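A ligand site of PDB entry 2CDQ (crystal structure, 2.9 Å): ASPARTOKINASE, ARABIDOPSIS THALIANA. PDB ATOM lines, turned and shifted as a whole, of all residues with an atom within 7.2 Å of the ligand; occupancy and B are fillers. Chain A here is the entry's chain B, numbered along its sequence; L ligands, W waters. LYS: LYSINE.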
ATOM      1  N   LYS A  32       0.640  10.617 -18.615  1.00  0.00           N
ATOM      2  CA  LYS A  32       1.358   9.369 -18.830  1.00  0.00           C
ATOM      3  C   LYS A  32       0.467   8.169 -18.515  1.00  0.00           C
ATOM      4  O   LYS A  32      -0.212   8.147 -17.486  1.00  0.00           O
ATOM      5  CB  LYS A  32       2.633   9.331 -17.988  1.00  0.00           C
ATOM      6  CG  LYS A  32       3.459   8.065 -18.143  1.00  0.00           C
ATOM      7  CD  LYS A  32       3.004   7.015 -17.146  1.00  0.00           C
ATOM      8  CE  LYS A  32       3.750   5.716 -17.314  1.00  0.00           C
ATOM      9  NZ  LYS A  32       3.728   4.987 -16.024  1.00  0.00           N
ATOM     10  N   PHE A  33       0.484   7.202 -19.423  1.00  0.00           N
ATOM     11  CA  PHE A  33      -0.332   5.988 -19.310  1.00  0.00           C
ATOM     12  C   PHE A  33       0.520   4.733 -19.436  1.00  0.00           C
ATOM     13  O   PHE A  33       1.288   4.591 -20.395  1.00  0.00           O
ATOM     14  CB  PHE A  33      -1.465   5.997 -20.342  1.00  0.00           C
ATOM     15  CG  PHE A  33      -2.488   7.054 -20.093  1.00  0.00           C
ATOM     16  CD1 PHE A  33      -3.586   6.797 -19.273  1.00  0.00           C
ATOM     17  CD2 PHE A  33      -2.353   8.327 -20.648  1.00  0.00           C
ATOM     18  CE1 PHE A  33      -4.536   7.776 -19.022  1.00  0.00           C
ATOM     19  CE2 PHE A  33      -3.295   9.329 -20.399  1.00  0.00           C
ATOM     20  CZ  PHE A  33      -4.392   9.048 -19.587  1.00  0.00           C
ATOM     21  N   GLY A  34       0.385   3.841 -18.463  1.00  0.00           N
ATOM     22  CA  GLY A  34       1.124   2.584 -18.430  1.00  0.00           C
ATOM     23  C   GLY A  34       0.564   1.521 -19.352  1.00  0.00           C
ATOM     24  O   GLY A  34      -0.467   1.720 -19.996  1.00  0.00           O
ATOM     25  N   GLY A  35       1.244   0.381 -19.415  1.00  0.00           N
ATOM     26  CA  GLY A  35       0.854  -0.729 -20.281  1.00  0.00           C
ATOM     27  C   GLY A  35      -0.603  -1.136 -20.184  1.00  0.00           C
ATOM     28  O   GLY A  35      -1.298  -1.231 -21.205  1.00  0.00           O
ATOM     29  N   SER A  36      -1.079  -1.384 -18.973  1.00  0.00           N
ATOM     30  CA  SER A  36      -2.437  -1.903 -18.778  1.00  0.00           C
ATOM     31  C   SER A  36      -3.558  -0.905 -19.115  1.00  0.00           C
ATOM     32  O   SER A  36      -4.671  -1.318 -19.442  1.00  0.00           O
ATOM     33  CB  SER A  36      -2.607  -2.450 -17.370  1.00  0.00           C
ATOM     34  OG  SER A  36      -2.938  -1.409 -16.480  1.00  0.00           O
ATOM     35  N   LEU A  63       2.697   7.395 -23.867  1.00  0.00           N
ATOM     36  CA  LEU A  63       2.222   6.013 -23.815  1.00  0.00           C
ATOM     37  C   LEU A  63       3.341   4.998 -23.692  1.00  0.00           C
ATOM     38  O   LEU A  63       4.407   5.136 -24.304  1.00  0.00           O
ATOM     39  CB  LEU A  63       1.383   5.671 -25.054  1.00  0.00           C
ATOM     40  CG  LEU A  63       0.073   6.425 -25.265  1.00  0.00           C
ATOM     41  CD1 LEU A  63      -0.595   5.883 -26.510  1.00  0.00           C
ATOM     42  CD2 LEU A  63      -0.840   6.299 -24.044  1.00  0.00           C
ATOM     43  N   SER A  64       3.074   3.954 -22.910  1.00  0.00           N
ATOM     44  CA  SER A  64       3.895   2.752 -22.872  1.00  0.00           C
ATOM     45  C   SER A  64       3.483   1.822 -24.001  1.00  0.00           C
ATOM     46  O   SER A  64       2.596   2.153 -24.791  1.00  0.00           O
ATOM     47  CB  SER A  64       3.719   2.050 -21.534  1.00  0.00           C
ATOM     48  OG  SER A  64       4.106   2.904 -20.471  1.00  0.00           O
ATOM     49  N   ALA A  65       4.143   0.666 -24.096  1.00  0.00           N
ATOM     50  CA  ALA A  65       3.718  -0.395 -25.015  1.00  0.00           C
ATOM     51  C   ALA A  65       2.376  -0.963 -24.553  1.00  0.00           C
ATOM     52  O   ALA A  65       1.965  -0.766 -23.409  1.00  0.00           O
ATOM     53  CB  ALA A  65       4.767  -1.473 -25.073  1.00  0.00           C
ATOM     54  N   MET A  66       1.685  -1.665 -25.447  1.00  0.00           N
ATOM     55  CA  MET A  66       0.400  -2.278 -25.120  1.00  0.00           C
ATOM     56  C   MET A  66       0.594  -3.429 -24.151  1.00  0.00           C
ATOM     57  O   MET A  66       1.262  -4.422 -24.474  1.00  0.00           O
ATOM     58  CB  MET A  66      -0.324  -2.749 -26.379  1.00  0.00           C
ATOM     59  CG  MET A  66      -0.765  -1.615 -27.283  1.00  0.00           C
ATOM     60  SD  MET A  66      -1.879  -2.189 -28.558  1.00  0.00           S
ATOM     61  CE  MET A  66      -3.389  -2.434 -27.617  1.00  0.00           C
ATOM     62  N   GLY A  67       0.007  -3.279 -22.957  1.00  0.00           N
ATOM     63  CA  GLY A  67       0.233  -4.153 -21.803  1.00  0.00           C
ATOM     64  C   GLY A  67       0.912  -5.472 -22.057  1.00  0.00           C
ATOM     65  O   GLY A  67       0.369  -6.335 -22.740  1.00  0.00           O
ATOM     66  N   LYS A  68       2.102  -5.620 -21.504  1.00  0.00           N
ATOM     67  CA  LYS A  68       2.876  -6.863 -21.592  1.00  0.00           C
ATOM     68  C   LYS A  68       3.635  -7.109 -22.925  1.00  0.00           C
ATOM     69  O   LYS A  68       4.383  -8.079 -23.022  1.00  0.00           O
ATOM     70  CB  LYS A  68       2.036  -8.088 -21.217  1.00  0.00           C
ATOM     71  CG  LYS A  68       1.904  -8.330 -19.737  1.00  0.00           C
ATOM     72  CD  LYS A  68       1.297  -9.696 -19.472  1.00  0.00           C
ATOM     73  CE  LYS A  68       0.915  -9.898 -18.000  1.00  0.00           C
ATOM     74  NZ  LYS A  68       2.071  -9.743 -17.071  1.00  0.00           N
ATOM     75  N   THR A  69       3.464  -6.240 -23.932  1.00  0.00           N
ATOM     76  CA  THR A  69       4.202  -6.447 -25.176  1.00  0.00           C
ATOM     77  C   THR A  69       5.696  -6.134 -25.052  1.00  0.00           C
ATOM     78  O   THR A  69       6.494  -6.701 -25.773  1.00  0.00           O
ATOM     79  CB  THR A  69       3.594  -5.744 -26.426  1.00  0.00           C
ATOM     80  OG1 THR A  69       3.351  -4.358 -26.146  1.00  0.00           O
ATOM     81  CG2 THR A  69       2.297  -6.415 -26.834  1.00  0.00           C
ATOM     82  N   THR A  70       6.062  -5.248 -24.132  1.00  0.00           N
ATOM     83  CA  THR A  70       7.479  -4.979 -23.869  1.00  0.00           C
ATOM     84  C   THR A  70       8.165  -6.219 -23.320  1.00  0.00           C
ATOM     85  O   THR A  70       9.228  -6.609 -23.810  1.00  0.00           O
ATOM     86  CB  THR A  70       7.694  -3.783 -22.941  1.00  0.00           C
ATOM     87  OG1 THR A  70       7.585  -2.569 -23.701  1.00  0.00           O
ATOM     88  CG2 THR A  70       9.073  -3.837 -22.300  1.00  0.00           C
ATOM     89  N   ASN A  71       7.551  -6.846 -22.331  1.00  0.00           N
ATOM     90  CA  ASN A  71       8.073  -8.094 -21.797  1.00  0.00           C
ATOM     91  C   ASN A  71       8.082  -9.191 -22.864  1.00  0.00           C
ATOM     92  O   ASN A  71       9.023  -9.975 -22.948  1.00  0.00           O
ATOM     93  CB  ASN A  71       7.272  -8.549 -20.584  1.00  0.00           C
ATOM     94  CG  ASN A  71       8.028  -9.570 -19.739  1.00  0.00           C
ATOM     95  OD1 ASN A  71       7.548 -10.683 -19.521  1.00  0.00           O
ATOM     96  ND2 ASN A  71       9.213  -9.194 -19.286  1.00  0.00           N
ATOM     97  N   VAL A 144      12.774  -3.671 -28.116  1.00  0.00           N
ATOM     98  CA  VAL A 144      11.698  -3.146 -27.268  1.00  0.00           C
ATOM     99  C   VAL A 144      11.038  -1.883 -27.821  1.00  0.00           C
ATOM    100  O   VAL A 144       9.848  -1.666 -27.589  1.00  0.00           O
ATOM    101  CB  VAL A 144      12.099  -2.946 -25.765  1.00  0.00           C
ATOM    102  CG1 VAL A 144      12.734  -4.205 -25.176  1.00  0.00           C
ATOM    103  CG2 VAL A 144      13.000  -1.756 -25.599  1.00  0.00           C
ATOM    104  N   GLY A 147       7.634  -1.806 -29.326  1.00  0.00           N
ATOM    105  CA  GLY A 147       6.528  -1.752 -28.379  1.00  0.00           C
ATOM    106  C   GLY A 147       5.785  -0.440 -28.357  1.00  0.00           C
ATOM    107  O   GLY A 147       4.644  -0.374 -28.816  1.00  0.00           O
ATOM    108  N   GLU A 148       6.428   0.601 -27.852  1.00  0.00           N
ATOM    109  CA  GLU A 148       5.787   1.927 -27.760  1.00  0.00           C
ATOM    110  C   GLU A 148       5.640   2.613 -29.119  1.00  0.00           C
ATOM    111  O   GLU A 148       4.770   3.483 -29.281  1.00  0.00           O
ATOM    112  CB  GLU A 148       6.453   2.833 -26.716  1.00  0.00           C
ATOM    113  CG  GLU A 148       7.882   2.465 -26.337  1.00  0.00           C
ATOM    114  CD  GLU A 148       7.946   1.294 -25.384  1.00  0.00           C
ATOM    115  OE1 GLU A 148       7.479   1.427 -24.237  1.00  0.00           O
ATOM    116  OE2 GLU A 148       8.460   0.230 -25.780  1.00  0.00           O
ATOM    117  N   SER A 151       2.373   1.255 -30.124  1.00  0.00           N
ATOM    118  CA  SER A 151       1.394   1.843 -29.204  1.00  0.00           C
ATOM    119  C   SER A 151       0.920   3.204 -29.651  1.00  0.00           C
ATOM    120  O   SER A 151      -0.257   3.379 -29.988  1.00  0.00           O
ATOM    121  CB  SER A 151       2.012   1.992 -27.825  1.00  0.00           C
ATOM    122  OG  SER A 151       1.612   0.917 -27.009  1.00  0.00           O
ATOM    123  N   GLY A 214       7.195   6.031 -24.923  1.00  0.00           N
ATOM    124  CA  GLY A 214       7.573   5.890 -23.537  1.00  0.00           C
ATOM    125  C   GLY A 214       9.057   5.946 -23.320  1.00  0.00           C
ATOM    126  O   GLY A 214       9.684   6.971 -23.588  1.00  0.00           O
ATOM    127  N   PHE A 215       9.637   4.858 -22.849  1.00  0.00           N
ATOM    128  CA  PHE A 215      11.013   4.938 -22.361  1.00  0.00           C
ATOM    129  C   PHE A 215      12.072   4.868 -23.455  1.00  0.00           C
ATOM    130  O   PHE A 215      12.866   3.929 -23.534  1.00  0.00           O
ATOM    131  CB  PHE A 215      11.251   4.030 -21.137  1.00  0.00           C
ATOM    132  CG  PHE A 215      11.380   2.548 -21.421  1.00  0.00           C
ATOM    133  CD1 PHE A 215      12.269   1.779 -20.669  1.00  0.00           C
ATOM    134  CD2 PHE A 215      10.608   1.922 -22.392  1.00  0.00           C
ATOM    135  CE1 PHE A 215      12.401   0.422 -20.885  1.00  0.00           C
ATOM    136  CE2 PHE A 215      10.752   0.541 -22.624  1.00  0.00           C
ATOM    137  CZ  PHE A 215      11.646  -0.202 -21.858  1.00  0.00           C
ATOM    138  N   GLY A 229      15.956   3.235 -19.146  1.00  0.00           N
ATOM    139  CA  GLY A 229      16.216   2.469 -17.919  1.00  0.00           C
ATOM    140  C   GLY A 229      15.017   2.426 -16.995  1.00  0.00           C
ATOM    141  O   GLY A 229      13.865   2.493 -17.444  1.00  0.00           O
ATOM    142  N   ARG A 230      15.282   2.311 -15.695  1.00  0.00           N
ATOM    143  CA  ARG A 230      14.222   2.266 -14.689  1.00  0.00           C
ATOM    144  C   ARG A 230      13.436   3.567 -14.693  1.00  0.00           C
ATOM    145  O   ARG A 230      13.955   4.625 -15.055  1.00  0.00           O
ATOM    146  CB  ARG A 230      14.810   2.013 -13.303  1.00  0.00           C
ATOM    147  CG  ARG A 230      15.229   0.577 -13.072  1.00  0.00           C
ATOM    148  CD  ARG A 230      16.212   0.459 -11.924  1.00  0.00           C
ATOM    149  NE  ARG A 230      16.780  -0.882 -11.777  1.00  0.00           N
ATOM    150  CZ  ARG A 230      16.125  -2.032 -12.000  1.00  0.00           C
ATOM    151  NH1 ARG A 230      14.857  -2.034 -12.361  1.00  0.00           N
ATOM    152  NH2 ARG A 230      16.759  -3.186 -11.835  1.00  0.00           N
ATOM    153  N   GLY A 231      12.176   3.479 -14.283  1.00  0.00           N
ATOM    154  CA  GLY A 231      11.282   4.630 -14.376  1.00  0.00           C
ATOM    155  C   GLY A 231      11.281   5.209 -15.777  1.00  0.00           C
ATOM    156  O   GLY A 231      11.588   6.385 -15.970  1.00  0.00           O
ATOM    157  N   GLY A 232      10.944   4.373 -16.753  1.00  0.00           N
ATOM    158  CA  GLY A 232      10.974   4.743 -18.156  1.00  0.00           C
ATOM    159  C   GLY A 232       9.970   5.814 -18.527  1.00  0.00           C
ATOM    160  O   GLY A 232      10.283   7.000 -18.479  1.00  0.00           O
ATOM    161  N   SER A 233       8.766   5.382 -18.889  1.00  0.00           N
ATOM    162  CA  SER A 233       7.711   6.292 -19.370  1.00  0.00           C
ATOM    163  C   SER A 233       7.438   7.445 -18.401  1.00  0.00           C
ATOM    164  O   SER A 233       7.142   8.570 -18.822  1.00  0.00           O
ATOM    165  CB  SER A 233       6.424   5.528 -19.673  1.00  0.00           C
ATOM    166  OG  SER A 233       6.652   4.482 -20.593  1.00  0.00           O
ATOM    167  N   ASP A 234       7.538   7.172 -17.094  1.00  0.00           N
ATOM    168  CA  ASP A 234       7.405   8.214 -16.077  1.00  0.00           C
ATOM    169  C   ASP A 234       8.435   9.336 -16.326  1.00  0.00           C
ATOM    170  O   ASP A 234       8.095  10.522 -16.310  1.00  0.00           O
ATOM    171  CB  ASP A 234       7.566   7.638 -14.656  1.00  0.00           C
ATOM    172  CG  ASP A 234       6.416   6.693 -14.258  1.00  0.00           C
ATOM    173  OD1 ASP A 234       5.322   6.749 -14.854  1.00  0.00           O
ATOM    174  OD2 ASP A 234       6.612   5.892 -13.324  1.00  0.00           O
ATOM    175  N   LEU A 235       9.687   8.943 -16.571  1.00  0.00           N
ATOM    176  CA  LEU A 235      10.755   9.890 -16.880  1.00  0.00           C
ATOM    177  C   LEU A 235      10.468  10.694 -18.151  1.00  0.00           C
ATOM    178  O   LEU A 235      10.711  11.897 -18.183  1.00  0.00           O
ATOM    179  CB  LEU A 235      12.099   9.176 -17.006  1.00  0.00           C
ATOM    180  CG  LEU A 235      13.373   9.993 -17.224  1.00  0.00           C
ATOM    181  CD1 LEU A 235      13.587  10.987 -16.089  1.00  0.00           C
ATOM    182  CD2 LEU A 235      14.576   9.074 -17.376  1.00  0.00           C
ATOM    183  N   GLN A 289       3.329   0.997  -8.475  1.00  0.00           N
ATOM    184  CA  GLN A 289       4.339   0.507  -9.400  1.00  0.00           C
ATOM    185  C   GLN A 289       4.778   1.607 -10.356  1.00  0.00           C
ATOM    186  O   GLN A 289       4.967   1.385 -11.555  1.00  0.00           O
ATOM    187  CB  GLN A 289       3.864  -0.737 -10.159  1.00  0.00           C
ATOM    188  CG  GLN A 289       4.225  -2.052  -9.470  1.00  0.00           C
ATOM    189  CD  GLN A 289       3.200  -2.479  -8.437  1.00  0.00           C
ATOM    190  OE1 GLN A 289       3.084  -1.871  -7.377  1.00  0.00           O
ATOM    191  NE2 GLN A 289       2.474  -3.544  -8.735  1.00  0.00           N
HETATM  192  N   LYS L   1       6.915   1.115 -21.520  1.00  0.00           N
HETATM  193  CA  LYS L   1       6.978  -0.380 -21.461  1.00  0.00           C
HETATM  194  C   LYS L   1       5.652  -1.033 -21.027  1.00  0.00           C
HETATM  195  O   LYS L   1       5.133  -1.888 -21.748  1.00  0.00           O
HETATM  196  CB  LYS L   1       8.149  -0.860 -20.574  1.00  0.00           C
HETATM  197  CG  LYS L   1       8.141  -0.406 -19.115  1.00  0.00           C
HETATM  198  CD  LYS L   1       8.509   1.062 -18.973  1.00  0.00           C
HETATM  199  CE  LYS L   1       8.194   1.564 -17.585  1.00  0.00           C
HETATM  200  NZ  LYS L   1       7.541   2.892 -17.678  1.00  0.00           N
HETATM  201  OXT LYS L   1       5.061  -0.736 -19.988  1.00  0.00           O
HETATM  202  O   HOH W   1       4.927   1.076 -17.805  1.00  0.00           O
HETATM  203  O   HOH W   2       3.907  -1.259 -17.707  1.00  0.00           O
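OG1 of Thr 70 sits close to O of the ligand, 3.2 Å away.
The side-chain carboxylate (OE1) of Glu 148 lies within salt-bridge range of a nitrogen (N) of the ligand, 2.8 Å away.
The side-chain hydroxyl (OG) of Ser 233 lies within hydrogen-bond range of a nitrogen (NZ) of the ligand, at 3.4 Å.
N of the ligand sits close to OG of Ser 64 (3.5 Å).
The side-chain hydroxyl of Ser 151 lies within hydrogen-bond range of the backbone carbonyl oxygen of Ser 64 (2.7 Å).
The side-chain hydroxyl (OG) of Ser 233 sits at hydrogen-bond distance from the side-chain hydroxyl (OG) of Ser 64 (3.0 Å).
The side-chain carboxylate (OE1) of Glu 148 sits at hydrogen-bond distance from the backbone NH (N) of Ala 65.
The backbone NH of Ser 64 is in hydrogen-bond range of the backbone carbonyl oxygen of Phe 33 (3.1 Å).
Water W1 bridges an oxygen (OXT) of the ligand (2.8 Å) and the side-chain hydroxyl (OG) of Ser 64 (3.3 Å).
Merely in contact with the ligand: Ala 65, Phe 215 and Gly 232.
Hydrophobic or aromatic side chains within 4 Å of the ligand: Ala 65 and Phe 215.
The nearest printed residue that does not touch the ligand is Gly 35 (4.02 Å).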
